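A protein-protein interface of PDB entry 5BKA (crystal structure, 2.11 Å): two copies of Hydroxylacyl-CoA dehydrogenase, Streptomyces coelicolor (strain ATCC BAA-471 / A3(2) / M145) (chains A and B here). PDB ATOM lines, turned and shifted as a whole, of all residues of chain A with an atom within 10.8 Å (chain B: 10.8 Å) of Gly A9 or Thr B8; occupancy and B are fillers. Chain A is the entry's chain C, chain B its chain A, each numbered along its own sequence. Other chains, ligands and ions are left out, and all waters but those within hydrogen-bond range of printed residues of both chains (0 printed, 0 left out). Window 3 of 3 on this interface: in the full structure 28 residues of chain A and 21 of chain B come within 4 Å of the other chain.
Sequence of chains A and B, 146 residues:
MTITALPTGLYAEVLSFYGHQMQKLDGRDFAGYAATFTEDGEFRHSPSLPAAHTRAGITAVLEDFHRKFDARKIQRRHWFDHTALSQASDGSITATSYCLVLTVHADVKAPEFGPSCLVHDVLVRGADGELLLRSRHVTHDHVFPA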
ATOM      1  N   GLY A   9      16.269   5.231 -26.650  1.00  0.00           N
ATOM      2  CA  GLY A   9      15.076   4.747 -27.322  1.00  0.00           C
ATOM      3  C   GLY A   9      15.166   3.286 -27.720  1.00  0.00           C
ATOM      4  O   GLY A   9      14.180   2.551 -27.655  1.00  0.00           O
ATOM      5  N   LEU A  10      16.361   2.867 -28.142  1.00  0.00           N
ATOM      6  CA  LEU A  10      16.570   1.471 -28.512  1.00  0.00           C
ATOM      7  C   LEU A  10      16.414   0.548 -27.309  1.00  0.00           C
ATOM      8  O   LEU A  10      15.874  -0.558 -27.434  1.00  0.00           O
ATOM      9  CB  LEU A  10      17.949   1.299 -29.147  1.00  0.00           C
ATOM     10  CG  LEU A  10      18.393  -0.142 -29.406  1.00  0.00           C
ATOM     11  CD1 LEU A  10      17.632  -0.738 -30.582  1.00  0.00           C
ATOM     12  CD2 LEU A  10      19.894  -0.211 -29.639  1.00  0.00           C
ATOM     13  N   TYR A  11      16.875   0.986 -26.135  1.00  0.00           N
ATOM     14  CA  TYR A  11      16.818   0.136 -24.949  1.00  0.00           C
ATOM     15  C   TYR A  11      15.377  -0.190 -24.573  1.00  0.00           C
ATOM     16  O   TYR A  11      15.044  -1.347 -24.294  1.00  0.00           O
ATOM     17  CB  TYR A  11      17.542   0.809 -23.783  1.00  0.00           C
ATOM     18  CG  TYR A  11      17.744  -0.103 -22.593  1.00  0.00           C
ATOM     19  CD1 TYR A  11      18.844  -0.947 -22.521  1.00  0.00           C
ATOM     20  CD2 TYR A  11      16.830  -0.127 -21.548  1.00  0.00           C
ATOM     21  CE1 TYR A  11      19.029  -1.786 -21.439  1.00  0.00           C
ATOM     22  CE2 TYR A  11      17.007  -0.963 -20.462  1.00  0.00           C
ATOM     23  CZ  TYR A  11      18.109  -1.791 -20.413  1.00  0.00           C
ATOM     24  OH  TYR A  11      18.290  -2.625 -19.334  1.00  0.00           O
ATOM     25  N   ALA A  12      14.509   0.823 -24.551  1.00  0.00           N
ATOM     26  CA  ALA A  12      13.099   0.580 -24.259  1.00  0.00           C
ATOM     27  C   ALA A  12      12.456  -0.307 -25.319  1.00  0.00           C
ATOM     28  O   ALA A  12      11.592  -1.135 -25.006  1.00  0.00           O
ATOM     29  CB  ALA A  12      12.349   1.907 -24.141  1.00  0.00           C
ATOM     30  N   GLU A  13      12.856  -0.143 -26.584  1.00  0.00           N
ATOM     31  CA  GLU A  13      12.307  -0.979 -27.648  1.00  0.00           C
ATOM     32  C   GLU A  13      12.701  -2.441 -27.472  1.00  0.00           C
ATOM     33  O   GLU A  13      11.899  -3.341 -27.749  1.00  0.00           O
ATOM     34  CB  GLU A  13      12.758  -0.464 -29.014  1.00  0.00           C
ATOM     35  CG  GLU A  13      11.866  -0.914 -30.160  1.00  0.00           C
ATOM     36  CD  GLU A  13      12.522  -0.741 -31.516  1.00  0.00           C
ATOM     37  OE1 GLU A  13      13.588  -0.095 -31.584  1.00  0.00           O
ATOM     38  OE2 GLU A  13      11.971  -1.253 -32.514  1.00  0.00           O
ATOM     39  N   VAL A  14      13.930  -2.698 -27.018  1.00  0.00           N
ATOM     40  CA  VAL A  14      14.371  -4.074 -26.803  1.00  0.00           C
ATOM     41  C   VAL A  14      13.605  -4.702 -25.644  1.00  0.00           C
ATOM     42  O   VAL A  14      13.195  -5.867 -25.713  1.00  0.00           O
ATOM     43  CB  VAL A  14      15.893  -4.117 -26.574  1.00  0.00           C
ATOM     44  CG1 VAL A  14      16.329  -5.505 -26.124  1.00  0.00           C
ATOM     45  CG2 VAL A  14      16.625  -3.712 -27.842  1.00  0.00           C
ATOM     46  N   LEU A  15      13.409  -3.945 -24.560  1.00  0.00           N
ATOM     47  CA  LEU A  15      12.584  -4.433 -23.459  1.00  0.00           C
ATOM     48  C   LEU A  15      11.171  -4.733 -23.937  1.00  0.00           C
ATOM     49  O   LEU A  15      10.580  -5.751 -23.556  1.00  0.00           O
ATOM     50  CB  LEU A  15      12.556  -3.408 -22.324  1.00  0.00           C
ATOM     51  CG  LEU A  15      13.843  -3.193 -21.526  1.00  0.00           C
ATOM     52  CD1 LEU A  15      13.582  -2.282 -20.336  1.00  0.00           C
ATOM     53  CD2 LEU A  15      14.420  -4.521 -21.071  1.00  0.00           C
ATOM     54  N   SER A  16      10.608  -3.843 -24.758  1.00  0.00           N
ATOM     55  CA  SER A  16       9.299  -4.091 -25.351  1.00  0.00           C
ATOM     56  C   SER A  16       9.328  -5.329 -26.240  1.00  0.00           C
ATOM     57  O   SER A  16       8.425  -6.171 -26.181  1.00  0.00           O
ATOM     58  CB  SER A  16       8.849  -2.865 -26.146  1.00  0.00           C
ATOM     59  OG  SER A  16       7.492  -2.977 -26.539  1.00  0.00           O
ATOM     60  N   PHE A  17      10.360  -5.445 -27.083  1.00  0.00           N
ATOM     61  CA  PHE A  17      10.535  -6.631 -27.915  1.00  0.00           C
ATOM     62  C   PHE A  17      10.524  -7.905 -27.076  1.00  0.00           C
ATOM     63  O   PHE A  17       9.836  -8.876 -27.406  1.00  0.00           O
ATOM     64  CB  PHE A  17      11.839  -6.515 -28.709  1.00  0.00           C
ATOM     65  CG  PHE A  17      12.176  -7.736 -29.520  1.00  0.00           C
ATOM     66  CD1 PHE A  17      11.535  -7.986 -30.723  1.00  0.00           C
ATOM     67  CD2 PHE A  17      13.141  -8.629 -29.083  1.00  0.00           C
ATOM     68  CE1 PHE A  17      11.847  -9.106 -31.472  1.00  0.00           C
ATOM     69  CE2 PHE A  17      13.456  -9.751 -29.827  1.00  0.00           C
ATOM     70  CZ  PHE A  17      12.808  -9.990 -31.023  1.00  0.00           C
ATOM     71  N   THR A  83      18.879  -6.357 -18.813  1.00  0.00           N
ATOM     72  CA  THR A  83      19.282  -6.335 -20.211  1.00  0.00           C
ATOM     73  C   THR A  83      20.398  -5.316 -20.408  1.00  0.00           C
ATOM     74  O   THR A  83      20.305  -4.179 -19.941  1.00  0.00           O
ATOM     75  CB  THR A  83      18.086  -5.997 -21.105  1.00  0.00           C
ATOM     76  OG1 THR A  83      17.117  -7.049 -21.027  1.00  0.00           O
ATOM     77  CG2 THR A  83      18.530  -5.835 -22.549  1.00  0.00           C
ATOM     78  N   LEU A  85      22.897  -3.885 -23.593  1.00  0.00           N
ATOM     79  CA  LEU A  85      23.123  -3.918 -25.027  1.00  0.00           C
ATOM     80  C   LEU A  85      24.532  -3.410 -25.296  1.00  0.00           C
ATOM     81  O   LEU A  85      25.051  -2.555 -24.566  1.00  0.00           O
ATOM     82  CB  LEU A  85      22.068  -3.084 -25.771  1.00  0.00           C
ATOM     83  CG  LEU A  85      20.649  -3.241 -25.206  1.00  0.00           C
ATOM     84  CD1 LEU A  85      19.745  -2.134 -25.715  1.00  0.00           C
ATOM     85  CD2 LEU A  85      20.087  -4.610 -25.566  1.00  0.00           C
ATOM     86  N   ILE A  93      23.094  -5.656 -32.938  1.00  0.00           N
ATOM     87  CA  ILE A  93      23.158  -5.365 -31.508  1.00  0.00           C
ATOM     88  C   ILE A  93      23.168  -6.651 -30.687  1.00  0.00           C
ATOM     89  O   ILE A  93      22.220  -7.443 -30.722  1.00  0.00           O
ATOM     90  CB  ILE A  93      21.996  -4.469 -31.075  1.00  0.00           C
ATOM     91  CG1 ILE A  93      21.994  -3.148 -31.852  1.00  0.00           C
ATOM     92  CG2 ILE A  93      22.073  -4.209 -29.580  1.00  0.00           C
ATOM     93  CD1 ILE A  93      23.016  -2.143 -31.356  1.00  0.00           C
ATOM     94  N   LEU A 123      20.795  -8.892 -32.019  1.00  0.00           N
ATOM     95  CA  LEU A 123      19.634  -8.199 -32.557  1.00  0.00           C
ATOM     96  C   LEU A 123      20.025  -7.524 -33.864  1.00  0.00           C
ATOM     97  O   LEU A 123      21.101  -6.930 -33.964  1.00  0.00           O
ATOM     98  CB  LEU A 123      19.114  -7.150 -31.572  1.00  0.00           C
ATOM     99  CG  LEU A 123      18.507  -7.615 -30.249  1.00  0.00           C
ATOM    100  CD1 LEU A 123      18.696  -6.533 -29.201  1.00  0.00           C
ATOM    101  CD2 LEU A 123      17.034  -7.947 -30.419  1.00  0.00           C
ATOM    102  N   ARG A 125      18.152  -5.441 -37.615  1.00  0.00           N
ATOM    103  CA  ARG A 125      17.051  -4.615 -38.085  1.00  0.00           C
ATOM    104  C   ARG A 125      16.269  -5.359 -39.157  1.00  0.00           C
ATOM    105  O   ARG A 125      16.855  -5.836 -40.139  1.00  0.00           O
ATOM    106  CB  ARG A 125      17.557  -3.290 -38.651  1.00  0.00           C
ATOM    107  CG  ARG A 125      16.497  -2.179 -38.702  1.00  0.00           C
ATOM    108  CD  ARG A 125      15.609  -2.290 -37.508  1.00  0.00           C
ATOM    109  NE  ARG A 125      16.310  -1.952 -36.265  1.00  0.00           N
ATOM    110  CZ  ARG A 125      15.706  -1.541 -35.153  1.00  0.00           C
ATOM    111  NH1 ARG A 125      14.384  -1.488 -35.111  1.00  0.00           N
ATOM    112  NH2 ARG A 125      16.415  -1.219 -34.077  1.00  0.00           N
ATOM    113  N   GLY A 129      11.425  -2.753 -40.517  1.00  0.00           N
ATOM    114  CA  GLY A 129      11.931  -1.932 -39.443  1.00  0.00           C
ATOM    115  C   GLY A 129      11.769  -2.531 -38.064  1.00  0.00           C
ATOM    116  O   GLY A 129      12.146  -1.884 -37.079  1.00  0.00           O
ATOM    117  N   LEU A 131      12.476  -5.185 -34.898  1.00  0.00           N
ATOM    118  CA  LEU A 131      13.616  -5.905 -34.357  1.00  0.00           C
ATOM    119  C   LEU A 131      13.450  -7.401 -34.592  1.00  0.00           C
ATOM    120  O   LEU A 131      12.337  -7.932 -34.602  1.00  0.00           O
ATOM    121  CB  LEU A 131      13.771  -5.628 -32.862  1.00  0.00           C
ATOM    122  CG  LEU A 131      14.444  -4.321 -32.444  1.00  0.00           C
ATOM    123  CD1 LEU A 131      14.353  -4.133 -30.934  1.00  0.00           C
ATOM    124  CD2 LEU A 131      15.892  -4.293 -32.903  1.00  0.00           C
ATOM    125  N   THR B   2       8.716   0.124 -36.296  1.00  0.00           N
ATOM    126  CA  THR B   2       7.774  -0.049 -37.397  1.00  0.00           C
ATOM    127  C   THR B   2       6.600   0.917 -37.255  1.00  0.00           C
ATOM    128  O   THR B   2       6.478   1.610 -36.247  1.00  0.00           O
ATOM    129  CB  THR B   2       7.259  -1.500 -37.475  1.00  0.00           C
ATOM    130  OG1 THR B   2       6.475  -1.670 -38.662  1.00  0.00           O
ATOM    131  CG2 THR B   2       6.417  -1.840 -36.255  1.00  0.00           C
ATOM    132  N   THR B   4       3.391   0.695 -36.812  1.00  0.00           N
ATOM    133  CA  THR B   4       2.363   0.491 -35.801  1.00  0.00           C
ATOM    134  C   THR B   4       2.915   0.513 -34.383  1.00  0.00           C
ATOM    135  O   THR B   4       2.137   0.437 -33.427  1.00  0.00           O
ATOM    136  CB  THR B   4       1.629  -0.830 -36.049  1.00  0.00           C
ATOM    137  OG1 THR B   4       0.852  -1.170 -34.893  1.00  0.00           O
ATOM    138  CG2 THR B   4       2.623  -1.943 -36.334  1.00  0.00           C
ATOM    139  N   ALA B   5       4.229   0.629 -34.220  1.00  0.00           N
ATOM    140  CA  ALA B   5       4.828   0.604 -32.895  1.00  0.00           C
ATOM    141  C   ALA B   5       4.511   1.883 -32.129  1.00  0.00           C
ATOM    142  O   ALA B   5       4.380   2.967 -32.704  1.00  0.00           O
ATOM    143  CB  ALA B   5       6.343   0.421 -32.997  1.00  0.00           C
ATOM    144  N   LEU B   6       4.379   1.741 -30.816  1.00  0.00           N
ATOM    145  CA  LEU B   6       4.159   2.869 -29.930  1.00  0.00           C
ATOM    146  C   LEU B   6       5.486   3.554 -29.614  1.00  0.00           C
ATOM    147  O   LEU B   6       6.554   2.955 -29.764  1.00  0.00           O
ATOM    148  CB  LEU B   6       3.480   2.397 -28.647  1.00  0.00           C
ATOM    149  CG  LEU B   6       1.963   2.204 -28.723  1.00  0.00           C
ATOM    150  CD1 LEU B   6       1.444   1.523 -27.466  1.00  0.00           C
ATOM    151  CD2 LEU B   6       1.262   3.535 -28.944  1.00  0.00           C
ATOM    152  N   PRO B   7       5.451   4.818 -29.189  1.00  0.00           N
ATOM    153  CA  PRO B   7       6.704   5.521 -28.880  1.00  0.00           C
ATOM    154  C   PRO B   7       7.441   4.876 -27.714  1.00  0.00           C
ATOM    155  O   PRO B   7       6.833   4.415 -26.745  1.00  0.00           O
ATOM    156  CB  PRO B   7       6.241   6.942 -28.539  1.00  0.00           C
ATOM    157  CG  PRO B   7       4.796   6.803 -28.182  1.00  0.00           C
ATOM    158  CD  PRO B   7       4.282   5.707 -29.061  1.00  0.00           C
ATOM    159  N   THR B   8       8.772   4.849 -27.822  1.00  0.00           N
ATOM    160  CA  THR B   8       9.592   4.243 -26.778  1.00  0.00           C
ATOM    161  C   THR B   8       9.542   5.043 -25.483  1.00  0.00           C
ATOM    162  O   THR B   8       9.630   4.462 -24.395  1.00  0.00           O
ATOM    163  CB  THR B   8      11.037   4.105 -27.256  1.00  0.00           C
ATOM    164  N   GLY B   9       9.411   6.369 -25.577  1.00  0.00           N
ATOM    165  CA  GLY B   9       9.285   7.178 -24.376  1.00  0.00           C
ATOM    166  C   GLY B   9       8.083   6.789 -23.538  1.00  0.00           C
ATOM    167  O   GLY B   9       8.133   6.828 -22.306  1.00  0.00           O
ATOM    168  N   LEU B  10       6.982   6.420 -24.196  1.00  0.00           N
ATOM    169  CA  LEU B  10       5.797   5.976 -23.471  1.00  0.00           C
ATOM    170  C   LEU B  10       6.070   4.682 -22.712  1.00  0.00           C
ATOM    171  O   LEU B  10       5.588   4.501 -21.588  1.00  0.00           O
ATOM    172  CB  LEU B  10       4.629   5.798 -24.442  1.00  0.00           C
ATOM    173  CG  LEU B  10       3.386   5.074 -23.925  1.00  0.00           C
ATOM    174  CD1 LEU B  10       2.682   5.901 -22.859  1.00  0.00           C
ATOM    175  CD2 LEU B  10       2.444   4.760 -25.076  1.00  0.00           C
ATOM    176  N   TYR B  11       6.845   3.772 -23.309  1.00  0.00           N
ATOM    177  CA  TYR B  11       7.131   2.497 -22.657  1.00  0.00           C
ATOM    178  C   TYR B  11       7.915   2.708 -21.367  1.00  0.00           C
ATOM    179  O   TYR B  11       7.585   2.131 -20.325  1.00  0.00           O
ATOM    180  CB  TYR B  11       7.894   1.576 -23.610  1.00  0.00           C
ATOM    181  CG  TYR B  11       8.062   0.164 -23.093  1.00  0.00           C
ATOM    182  CD1 TYR B  11       7.075  -0.793 -23.296  1.00  0.00           C
ATOM    183  CD2 TYR B  11       9.206  -0.213 -22.402  1.00  0.00           C
ATOM    184  CE1 TYR B  11       7.223  -2.087 -22.826  1.00  0.00           C
ATOM    185  CE2 TYR B  11       9.363  -1.503 -21.927  1.00  0.00           C
ATOM    186  CZ  TYR B  11       8.369  -2.435 -22.142  1.00  0.00           C
ATOM    187  OH  TYR B  11       8.523  -3.719 -21.670  1.00  0.00           O
ATOM    188  N   ALA B  12       8.964   3.532 -21.423  1.00  0.00           N
ATOM    189  CA  ALA B  12       9.722   3.846 -20.215  1.00  0.00           C
ATOM    190  C   ALA B  12       8.851   4.568 -19.196  1.00  0.00           C
ATOM    191  O   ALA B  12       8.998   4.361 -17.985  1.00  0.00           O
ATOM    192  CB  ALA B  12      10.949   4.687 -20.568  1.00  0.00           C
ATOM    193  N   GLU B  13       7.937   5.418 -19.668  1.00  0.00           N
ATOM    194  CA  GLU B  13       7.039   6.124 -18.761  1.00  0.00           C
ATOM    195  C   GLU B  13       6.131   5.152 -18.019  1.00  0.00           C
ATOM    196  O   GLU B  13       5.816   5.359 -16.840  1.00  0.00           O
ATOM    197  CB  GLU B  13       6.210   7.151 -19.533  1.00  0.00           C
ATOM    198  N   VAL B  14       5.695   4.087 -18.695  1.00  0.00           N
ATOM    199  CA  VAL B  14       4.844   3.095 -18.047  1.00  0.00           C
ATOM    200  C   VAL B  14       5.626   2.335 -16.982  1.00  0.00           C
ATOM    201  O   VAL B  14       5.121   2.090 -15.880  1.00  0.00           O
ATOM    202  CB  VAL B  14       4.245   2.144 -19.098  1.00  0.00           C
ATOM    203  CG1 VAL B  14       3.483   1.011 -18.426  1.00  0.00           C
ATOM    204  CG2 VAL B  14       3.346   2.910 -20.053  1.00  0.00           C
ATOM    205  N   LEU B  15       6.868   1.953 -17.292  1.00  0.00           N
ATOM    206  CA  LEU B  15       7.709   1.281 -16.305  1.00  0.00           C
ATOM    207  C   LEU B  15       7.941   2.162 -15.082  1.00  0.00           C
ATOM    208  O   LEU B  15       7.854   1.690 -13.943  1.00  0.00           O
ATOM    209  CB  LEU B  15       9.041   0.882 -16.937  1.00  0.00           C
ATOM    210  CG  LEU B  15       9.002  -0.176 -18.042  1.00  0.00           C
ATOM    211  CD1 LEU B  15      10.413  -0.607 -18.417  1.00  0.00           C
ATOM    212  CD2 LEU B  15       8.167  -1.372 -17.616  1.00  0.00           C
ATOM    213  N   SER B  16       8.247   3.444 -15.298  1.00  0.00           N
ATOM    214  CA  SER B  16       8.397   4.369 -14.179  1.00  0.00           C
ATOM    215  C   SER B  16       7.094   4.500 -13.402  1.00  0.00           C
ATOM    216  O   SER B  16       7.098   4.503 -12.164  1.00  0.00           O
ATOM    217  CB  SER B  16       8.866   5.735 -14.681  1.00  0.00           C
ATOM    218  OG  SER B  16       8.728   6.721 -13.672  1.00  0.00           O
ATOM    219  N   THR B  83       6.407  -6.090 -19.444  1.00  0.00           N
ATOM    220  CA  THR B  83       5.294  -5.231 -19.836  1.00  0.00           C
ATOM    221  C   THR B  83       5.163  -5.181 -21.358  1.00  0.00           C
ATOM    222  O   THR B  83       6.162  -5.032 -22.071  1.00  0.00           O
ATOM    223  CB  THR B  83       5.492  -3.824 -19.271  1.00  0.00           C
ATOM    224  OG1 THR B  83       5.490  -3.872 -17.839  1.00  0.00           O
ATOM    225  CG2 THR B  83       4.386  -2.898 -19.744  1.00  0.00           C
ATOM    226  N   LEU B  85       2.551  -3.401 -24.314  1.00  0.00           N
ATOM    227  CA  LEU B  85       1.564  -2.359 -24.566  1.00  0.00           C
ATOM    228  C   LEU B  85       0.978  -2.474 -25.969  1.00  0.00           C
ATOM    229  O   LEU B  85       1.581  -3.037 -26.903  1.00  0.00           O
ATOM    230  CB  LEU B  85       2.152  -0.950 -24.365  1.00  0.00           C
ATOM    231  CG  LEU B  85       3.024  -0.680 -23.136  1.00  0.00           C
ATOM    232  CD1 LEU B  85       3.716   0.679 -23.254  1.00  0.00           C
ATOM    233  CD2 LEU B  85       2.259  -0.767 -21.833  1.00  0.00           C
ATOM    234  N   LEU B 131      -0.349   9.604 -16.171  1.00  0.00           N
ATOM    235  CA  LEU B 131      -0.849   8.308 -16.594  1.00  0.00           C
ATOM    236  C   LEU B 131      -1.787   7.754 -15.519  1.00  0.00           C
ATOM    237  O   LEU B 131      -1.435   7.859 -14.338  1.00  0.00           O
ATOM    238  CB  LEU B 131       0.341   7.358 -16.811  1.00  0.00           C
ATOM    239  CG  LEU B 131       1.100   7.521 -18.147  1.00  0.00           C
ATOM    240  CD1 LEU B 131       2.273   6.556 -18.204  1.00  0.00           C
ATOM    241  CD2 LEU B 131       0.156   7.307 -19.301  1.00  0.00           C
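The side-chain hydroxyl (OH) of Tyr B11 lies within hydrogen-bond range of the backbone carbonyl oxygen (O) of Leu A15.
Among the printed residues, pairs that only touch across the chains: Gly A9 with Thr B8, Ala A12 with Thr B8, Ala A12 with Tyr B11 and Ser A16 with Tyr B11.
The backbone carbonyl oxygen (O) of Thr B83 is in hydrogen-bond range of the side-chain hydroxyl (OH) of Tyr B11 (2.7 Å).
Ala A12 touches Tyr B11, but with the chains exchanged Tyr A11 does not touch Ala B12 (7.7 Å).
Leu A15 touches Tyr B11, but with the chains exchanged Tyr A11 does not touch Leu B15 (6.9 Å).
Ser A16 touches Tyr B11, but with the chains exchanged Tyr A11 does not touch Ser B16 (11.1 Å).
Positions printed for both chains: 9, 10, 11, 12, 13, 14, 15, 16, 83, 85 and 131.
Of the 5 pairs that touch across the chains among the printed residues, none has its exchanged pair printed and touching as well.
Gly A9 touches just one residue of chain B: Thr B8.
Thr B8 touches just these residues of chain A: Gly A9 and Ala A12.
No residue of chain B comes within 4 Å of Leu A10.
Ala A12 touches just these residues of chain B: Thr B8 and Tyr B11.
No residue of chain B comes within 4 Å of Glu A13.
No residue of chain A comes within 4 Å of Pro B7.
No residue of chain A comes within 4 Å of Gly B9.
No residue of chain A comes within 4 Å of Ala B12.
Printed residues of chain A within 4 Å of Tyr B11: Ala A12, Leu A15 and Ser A16.
Printed residues of chain B within 4 Å of Ser A16: Tyr B11.
Of the printed residues of chain B, Leu A15 touches Tyr B11 (3.5 Å).
Leu B85 touches none of the printed residues of chain A.
Printed residues of chain B that touch a printed residue of chain A: Thr B8 and Tyr B11.
Hydrophobic or aromatic side chains of chain B that line the printed part of chain A: Tyr B11.
Along chain B the printed residues that touch a printed residue of chain A span positions 8 to 11.
Printed residues of chain A that touch a printed residue of chain B: Gly A9, Ala A12, Leu A15 and Ser A16.
Among the printed residues, 5 pairs touch across the chains.
Among the printed residues, no Asp or Glu carboxylate lies within 4 Å of a Lys or Arg side-chain nitrogen of the other chain.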
